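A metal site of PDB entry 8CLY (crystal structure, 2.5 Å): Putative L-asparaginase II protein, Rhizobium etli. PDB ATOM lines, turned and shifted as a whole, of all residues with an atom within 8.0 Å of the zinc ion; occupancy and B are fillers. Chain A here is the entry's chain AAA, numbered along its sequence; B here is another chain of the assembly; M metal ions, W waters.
A ring nitrogen (NE2) of His 144 lies close to the side-chain sulfur (SG) of Cys 194 (3.1 Å).
NZ of Lys 56 sits close to SG of Cys 140 (3.2 Å).
The side-chain sulfur (SG) of Cys 140 lies close to the side-chain amide nitrogen (ND2) of Asn 139 (3.4 Å).
N of Cys 140 sits at hydrogen-bond distance from OD1 of Asn 138 (2.9 Å).
The guanidinium group (NE) of Arg 52 lies within salt-bridge range of the side-chain carboxylate (OD1) of Asp 192 (2.9 Å).
Merely in contact with the zinc ion: Asp 192 (3.8 Å).
Within 4 Å of the zinc ion: Cys 140, Lys 143, Asp 192 and Cys 194.
Along chain A the residues within 4 Å of the zinc ion span positions 140 to 194.
The side-chain sulfur (SG) of Cys 194 is bound to the zinc ion, 2.3 Å away.
NZ of Lys 143 binds the zinc ion, 2.4 Å away.
Water W1 binds the zinc ion (2.5 Å).
The side-chain sulfur (SG) of Cys 140 is bound to the zinc ion (2.5 Å).
The zinc ion has four donor atoms within binding distance.
Water W1 lies within hydrogen-bond range of the side-chain hydroxyl of Ser 53 (2.6 Å) and the side-chain carboxylate of Asp 192 (2.6 Å).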
ATOM      1  N   ARG A  52     -34.263 -23.544  10.558  1.00  0.00           N
ATOM      2  CA  ARG A  52     -33.092 -22.994  11.304  1.00  0.00           C
ATOM      3  C   ARG A  52     -33.204 -23.457  12.766  1.00  0.00           C
ATOM      4  O   ARG A  52     -33.445 -24.650  12.977  1.00  0.00           O
ATOM      5  CB  ARG A  52     -33.042 -21.465  11.150  1.00  0.00           C
ATOM      6  CG  ARG A  52     -33.135 -20.982   9.704  1.00  0.00           C
ATOM      7  CD  ARG A  52     -31.930 -21.311   8.839  1.00  0.00           C
ATOM      8  NE  ARG A  52     -30.771 -20.710   9.457  1.00  0.00           N
ATOM      9  CZ  ARG A  52     -30.459 -19.402   9.434  1.00  0.00           C
ATOM     10  NH1 ARG A  52     -31.174 -18.519   8.739  1.00  0.00           N
ATOM     11  NH2 ARG A  52     -29.439 -18.975  10.139  1.00  0.00           N
ATOM     12  N   SER A  53     -33.088 -22.540  13.731  1.00  0.00           N
ATOM     13  CA  SER A  53     -33.079 -22.818  15.185  1.00  0.00           C
ATOM     14  C   SER A  53     -34.443 -23.216  15.759  1.00  0.00           C
ATOM     15  O   SER A  53     -34.461 -23.675  16.936  1.00  0.00           O
ATOM     16  CB  SER A  53     -32.543 -21.639  15.905  1.00  0.00           C
ATOM     17  OG  SER A  53     -31.131 -21.765  15.957  1.00  0.00           O
ATOM     18  N   LYS A  56     -34.798 -26.993  17.165  1.00  0.00           N
ATOM     19  CA  LYS A  56     -33.727 -27.416  18.102  1.00  0.00           C
ATOM     20  C   LYS A  56     -34.207 -28.563  19.010  1.00  0.00           C
ATOM     21  O   LYS A  56     -33.389 -29.440  19.367  1.00  0.00           O
ATOM     22  CB  LYS A  56     -33.247 -26.196  18.883  1.00  0.00           C
ATOM     23  CG  LYS A  56     -32.137 -25.438  18.180  1.00  0.00           C
ATOM     24  CD  LYS A  56     -31.565 -24.277  18.969  1.00  0.00           C
ATOM     25  CE  LYS A  56     -30.401 -23.663  18.209  1.00  0.00           C
ATOM     26  NZ  LYS A  56     -30.043 -22.323  18.719  1.00  0.00           N
ATOM     27  N   GLN A  59     -33.698 -31.776  17.370  1.00  0.00           N
ATOM     28  CA  GLN A  59     -32.256 -32.110  17.210  1.00  0.00           C
ATOM     29  C   GLN A  59     -31.682 -32.513  18.578  1.00  0.00           C
ATOM     30  O   GLN A  59     -30.572 -33.054  18.610  1.00  0.00           O
ATOM     31  CB  GLN A  59     -31.492 -30.915  16.649  1.00  0.00           C
ATOM     32  CG  GLN A  59     -31.945 -30.484  15.268  1.00  0.00           C
ATOM     33  CD  GLN A  59     -31.410 -29.103  14.933  1.00  0.00           C
ATOM     34  OE1 GLN A  59     -31.456 -28.169  15.732  1.00  0.00           O
ATOM     35  NE2 GLN A  59     -30.871 -28.972  13.743  1.00  0.00           N
ATOM     36  N   ALA A  84     -32.079 -24.469  22.763  1.00  0.00           N
ATOM     37  CA  ALA A  84     -32.157 -22.993  22.940  1.00  0.00           C
ATOM     38  C   ALA A  84     -31.365 -22.162  21.947  1.00  0.00           C
ATOM     39  O   ALA A  84     -30.253 -22.567  21.585  1.00  0.00           O
ATOM     40  CB  ALA A  84     -31.679 -22.641  24.299  1.00  0.00           C
ATOM     41  N   SER A  85     -31.937 -21.015  21.572  1.00  0.00           N
ATOM     42  CA  SER A  85     -31.159 -19.947  20.870  1.00  0.00           C
ATOM     43  C   SER A  85     -30.985 -18.835  21.920  1.00  0.00           C
ATOM     44  O   SER A  85     -31.826 -17.914  21.961  1.00  0.00           O
ATOM     45  CB  SER A  85     -31.823 -19.461  19.611  1.00  0.00           C
ATOM     46  OG  SER A  85     -31.988 -20.524  18.692  1.00  0.00           O
ATOM     47  N   CYS A 112     -19.004 -24.231  16.642  1.00  0.00           N
ATOM     48  CA  CYS A 112     -20.112 -23.331  16.237  1.00  0.00           C
ATOM     49  C   CYS A 112     -19.591 -21.923  15.965  1.00  0.00           C
ATOM     50  O   CYS A 112     -20.284 -21.129  15.268  1.00  0.00           O
ATOM     51  CB  CYS A 112     -21.194 -23.281  17.308  1.00  0.00           C
ATOM     52  SG  CYS A 112     -20.605 -22.928  18.982  1.00  0.00           S
ATOM     53  N   ASN A 138     -22.061 -18.288  21.945  1.00  0.00           N
ATOM     54  CA  ASN A 138     -22.880 -18.649  20.772  1.00  0.00           C
ATOM     55  C   ASN A 138     -24.245 -19.113  21.270  1.00  0.00           C
ATOM     56  O   ASN A 138     -24.285 -19.964  22.170  1.00  0.00           O
ATOM     57  CB  ASN A 138     -22.192 -19.722  19.931  1.00  0.00           C
ATOM     58  CG  ASN A 138     -22.807 -19.878  18.550  1.00  0.00           C
ATOM     59  OD1 ASN A 138     -24.002 -20.142  18.431  1.00  0.00           O
ATOM     60  ND2 ASN A 138     -21.989 -19.727  17.516  1.00  0.00           N
ATOM     61  N   ASN A 139     -25.316 -18.580  20.674  1.00  0.00           N
ATOM     62  CA  ASN A 139     -26.724 -18.888  20.991  1.00  0.00           C
ATOM     63  C   ASN A 139     -26.971 -20.397  20.856  1.00  0.00           C
ATOM     64  O   ASN A 139     -27.904 -20.903  21.523  1.00  0.00           O
ATOM     65  CB  ASN A 139     -27.693 -18.070  20.146  1.00  0.00           C
ATOM     66  CG  ASN A 139     -27.775 -18.528  18.698  1.00  0.00           C
ATOM     67  OD1 ASN A 139     -26.904 -18.208  17.889  1.00  0.00           O
ATOM     68  ND2 ASN A 139     -28.819 -19.269  18.374  1.00  0.00           N
ATOM     69  N   CYS A 140     -26.164 -21.103  20.058  1.00  0.00           N
ATOM     70  CA  CYS A 140     -26.326 -22.566  19.841  1.00  0.00           C
ATOM     71  C   CYS A 140     -25.398 -23.390  20.734  1.00  0.00           C
ATOM     72  O   CYS A 140     -25.363 -24.617  20.556  1.00  0.00           O
ATOM     73  CB  CYS A 140     -26.043 -22.898  18.373  1.00  0.00           C
ATOM     74  SG  CYS A 140     -27.225 -22.091  17.243  1.00  0.00           S
ATOM     75  N   SER A 141     -24.681 -22.783  21.686  1.00  0.00           N
ATOM     76  CA  SER A 141     -23.674 -23.490  22.524  1.00  0.00           C
ATOM     77  C   SER A 141     -24.341 -24.613  23.339  1.00  0.00           C
ATOM     78  O   SER A 141     -23.650 -25.605  23.611  1.00  0.00           O
ATOM     79  CB  SER A 141     -22.889 -22.547  23.422  1.00  0.00           C
ATOM     80  OG  SER A 141     -23.690 -21.988  24.435  1.00  0.00           O
ATOM     81  N   LYS A 143     -27.095 -26.508  22.400  1.00  0.00           N
ATOM     82  CA  LYS A 143     -27.419 -27.546  21.402  1.00  0.00           C
ATOM     83  C   LYS A 143     -26.146 -28.316  21.064  1.00  0.00           C
ATOM     84  O   LYS A 143     -26.222 -29.555  20.969  1.00  0.00           O
ATOM     85  CB  LYS A 143     -28.051 -26.911  20.160  1.00  0.00           C
ATOM     86  CG  LYS A 143     -28.182 -27.895  19.006  1.00  0.00           C
ATOM     87  CD  LYS A 143     -28.829 -27.307  17.796  1.00  0.00           C
ATOM     88  CE  LYS A 143     -27.944 -26.283  17.129  1.00  0.00           C
ATOM     89  NZ  LYS A 143     -28.597 -25.764  15.912  1.00  0.00           N
ATOM     90  N   HIS A 144     -25.038 -27.581  20.884  1.00  0.00           N
ATOM     91  CA  HIS A 144     -23.737 -28.166  20.469  1.00  0.00           C
ATOM     92  C   HIS A 144     -23.148 -28.977  21.630  1.00  0.00           C
ATOM     93  O   HIS A 144     -22.634 -30.065  21.362  1.00  0.00           O
ATOM     94  CB  HIS A 144     -22.789 -27.096  19.910  1.00  0.00           C
ATOM     95  CG  HIS A 144     -23.168 -26.675  18.537  1.00  0.00           C
ATOM     96  ND1 HIS A 144     -22.257 -26.635  17.502  1.00  0.00           N
ATOM     97  CD2 HIS A 144     -24.345 -26.265  18.028  1.00  0.00           C
ATOM     98  CE1 HIS A 144     -22.860 -26.204  16.415  1.00  0.00           C
ATOM     99  NE2 HIS A 144     -24.149 -25.965  16.706  1.00  0.00           N
ATOM    100  N   PHE A 147     -24.956 -32.155  21.618  1.00  0.00           N
ATOM    101  CA  PHE A 147     -24.435 -32.957  20.487  1.00  0.00           C
ATOM    102  C   PHE A 147     -23.149 -33.679  20.897  1.00  0.00           C
ATOM    103  O   PHE A 147     -22.978 -34.901  20.621  1.00  0.00           O
ATOM    104  CB  PHE A 147     -24.160 -32.060  19.270  1.00  0.00           C
ATOM    105  CG  PHE A 147     -25.375 -31.558  18.509  1.00  0.00           C
ATOM    106  CD1 PHE A 147     -26.649 -32.059  18.752  1.00  0.00           C
ATOM    107  CD2 PHE A 147     -25.201 -30.633  17.492  1.00  0.00           C
ATOM    108  CE1 PHE A 147     -27.732 -31.608  18.010  1.00  0.00           C
ATOM    109  CE2 PHE A 147     -26.282 -30.202  16.741  1.00  0.00           C
ATOM    110  CZ  PHE A 147     -27.550 -30.671  17.013  1.00  0.00           C
ATOM    111  N   ASP A 192     -26.101 -23.900   8.458  1.00  0.00           N
ATOM    112  CA  ASP A 192     -26.760 -23.059   9.490  1.00  0.00           C
ATOM    113  C   ASP A 192     -25.756 -22.010  10.004  1.00  0.00           C
ATOM    114  O   ASP A 192     -24.581 -22.107   9.669  1.00  0.00           O
ATOM    115  CB  ASP A 192     -27.252 -23.918  10.652  1.00  0.00           C
ATOM    116  CG  ASP A 192     -28.571 -23.502  11.273  1.00  0.00           C
ATOM    117  OD1 ASP A 192     -29.027 -22.362  11.011  1.00  0.00           O
ATOM    118  OD2 ASP A 192     -29.128 -24.344  12.020  1.00  0.00           O
ATOM    119  N   GLY A 193     -26.216 -21.052  10.790  1.00  0.00           N
ATOM    120  CA  GLY A 193     -25.359 -20.087  11.506  1.00  0.00           C
ATOM    121  C   GLY A 193     -24.246 -20.782  12.247  1.00  0.00           C
ATOM    122  O   GLY A 193     -23.076 -20.276  12.263  1.00  0.00           O
ATOM    123  N   CYS A 194     -24.538 -21.934  12.864  1.00  0.00           N
ATOM    124  CA  CYS A 194     -23.601 -22.643  13.774  1.00  0.00           C
ATOM    125  C   CYS A 194     -22.836 -23.751  13.027  1.00  0.00           C
ATOM    126  O   CYS A 194     -22.244 -24.580  13.708  1.00  0.00           O
ATOM    127  CB  CYS A 194     -24.371 -23.233  14.936  1.00  0.00           C
ATOM    128  SG  CYS A 194     -25.560 -24.467  14.374  1.00  0.00           S
ATOM    129  N   SER A 195     -22.872 -23.719  11.684  1.00  0.00           N
ATOM    130  CA  SER A 195     -22.075 -24.578  10.759  1.00  0.00           C
ATOM    131  C   SER A 195     -22.615 -26.020  10.711  1.00  0.00           C
ATOM    132  O   SER A 195     -21.949 -26.853  10.052  1.00  0.00           O
ATOM    133  CB  SER A 195     -20.602 -24.531  11.101  1.00  0.00           C
ATOM    134  OG  SER A 195     -20.059 -23.227  10.975  1.00  0.00           O
ATOM    135  N   ILE A 196     -23.754 -26.325  11.325  1.00  0.00           N
ATOM    136  CA  ILE A 196     -24.415 -27.662  11.167  1.00  0.00           C
ATOM    137  C   ILE A 196     -25.377 -27.607   9.989  1.00  0.00           C
ATOM    138  O   ILE A 196     -25.817 -26.528   9.602  1.00  0.00           O
ATOM    139  CB  ILE A 196     -25.128 -28.134  12.464  1.00  0.00           C
ATOM    140  CG1 ILE A 196     -26.491 -27.452  12.663  1.00  0.00           C
ATOM    141  CG2 ILE A 196     -24.230 -27.969  13.689  1.00  0.00           C
ATOM    142  CD1 ILE A 196     -27.354 -28.121  13.688  1.00  0.00           C
ATOM    143  N   PRO A 197     -25.813 -28.764   9.433  1.00  0.00           N
ATOM    144  CA  PRO A 197     -26.866 -28.773   8.433  1.00  0.00           C
ATOM    145  C   PRO A 197     -28.193 -28.212   8.980  1.00  0.00           C
ATOM    146  O   PRO A 197     -28.570 -28.527  10.125  1.00  0.00           O
ATOM    147  CB  PRO A 197     -27.054 -30.256   8.054  1.00  0.00           C
ATOM    148  CG  PRO A 197     -25.839 -30.954   8.581  1.00  0.00           C
ATOM    149  CD  PRO A 197     -25.365 -30.121   9.757  1.00  0.00           C
ATOM    150  N   THR A 198     -28.878 -27.458   8.139  1.00  0.00           N
ATOM    151  CA  THR A 198     -30.308 -27.106   8.290  1.00  0.00           C
ATOM    152  C   THR A 198     -31.022 -27.520   7.004  1.00  0.00           C
ATOM    153  O   THR A 198     -30.472 -27.262   5.896  1.00  0.00           O
ATOM    154  CB  THR A 198     -30.480 -25.615   8.641  1.00  0.00           C
ATOM    155  OG1 THR A 198     -31.889 -25.398   8.781  1.00  0.00           O
ATOM    156  CG2 THR A 198     -29.889 -24.694   7.599  1.00  0.00           C
ATOM    157  N   TRP B 325     -20.795 -17.590  11.639  1.00  0.00           N
ATOM    158  CA  TRP B 325     -19.861 -17.217  12.742  1.00  0.00           C
ATOM    159  C   TRP B 325     -18.453 -17.766  12.489  1.00  0.00           C
ATOM    160  O   TRP B 325     -17.518 -17.108  12.916  1.00  0.00           O
ATOM    161  CB  TRP B 325     -20.433 -17.676  14.101  1.00  0.00           C
ATOM    162  CG  TRP B 325     -21.827 -17.187  14.348  1.00  0.00           C
ATOM    163  CD1 TRP B 325     -22.947 -17.936  14.576  1.00  0.00           C
ATOM    164  CD2 TRP B 325     -22.264 -15.820  14.330  1.00  0.00           C
ATOM    165  NE1 TRP B 325     -24.043 -17.135  14.717  1.00  0.00           N
ATOM    166  CE2 TRP B 325     -23.660 -15.826  14.564  1.00  0.00           C
ATOM    167  CE3 TRP B 325     -21.612 -14.585  14.134  1.00  0.00           C
ATOM    168  CZ2 TRP B 325     -24.406 -14.658  14.622  1.00  0.00           C
ATOM    169  CZ3 TRP B 325     -22.362 -13.429  14.185  1.00  0.00           C
ATOM    170  CH2 TRP B 325     -23.741 -13.466  14.450  1.00  0.00           C
HETATM  171 ZN    ZN M   1     -27.471 -23.677  15.324  1.00  0.00          ZN
HETATM  172  O   HOH W   1     -29.510 -22.874  14.191  1.00  0.00           O
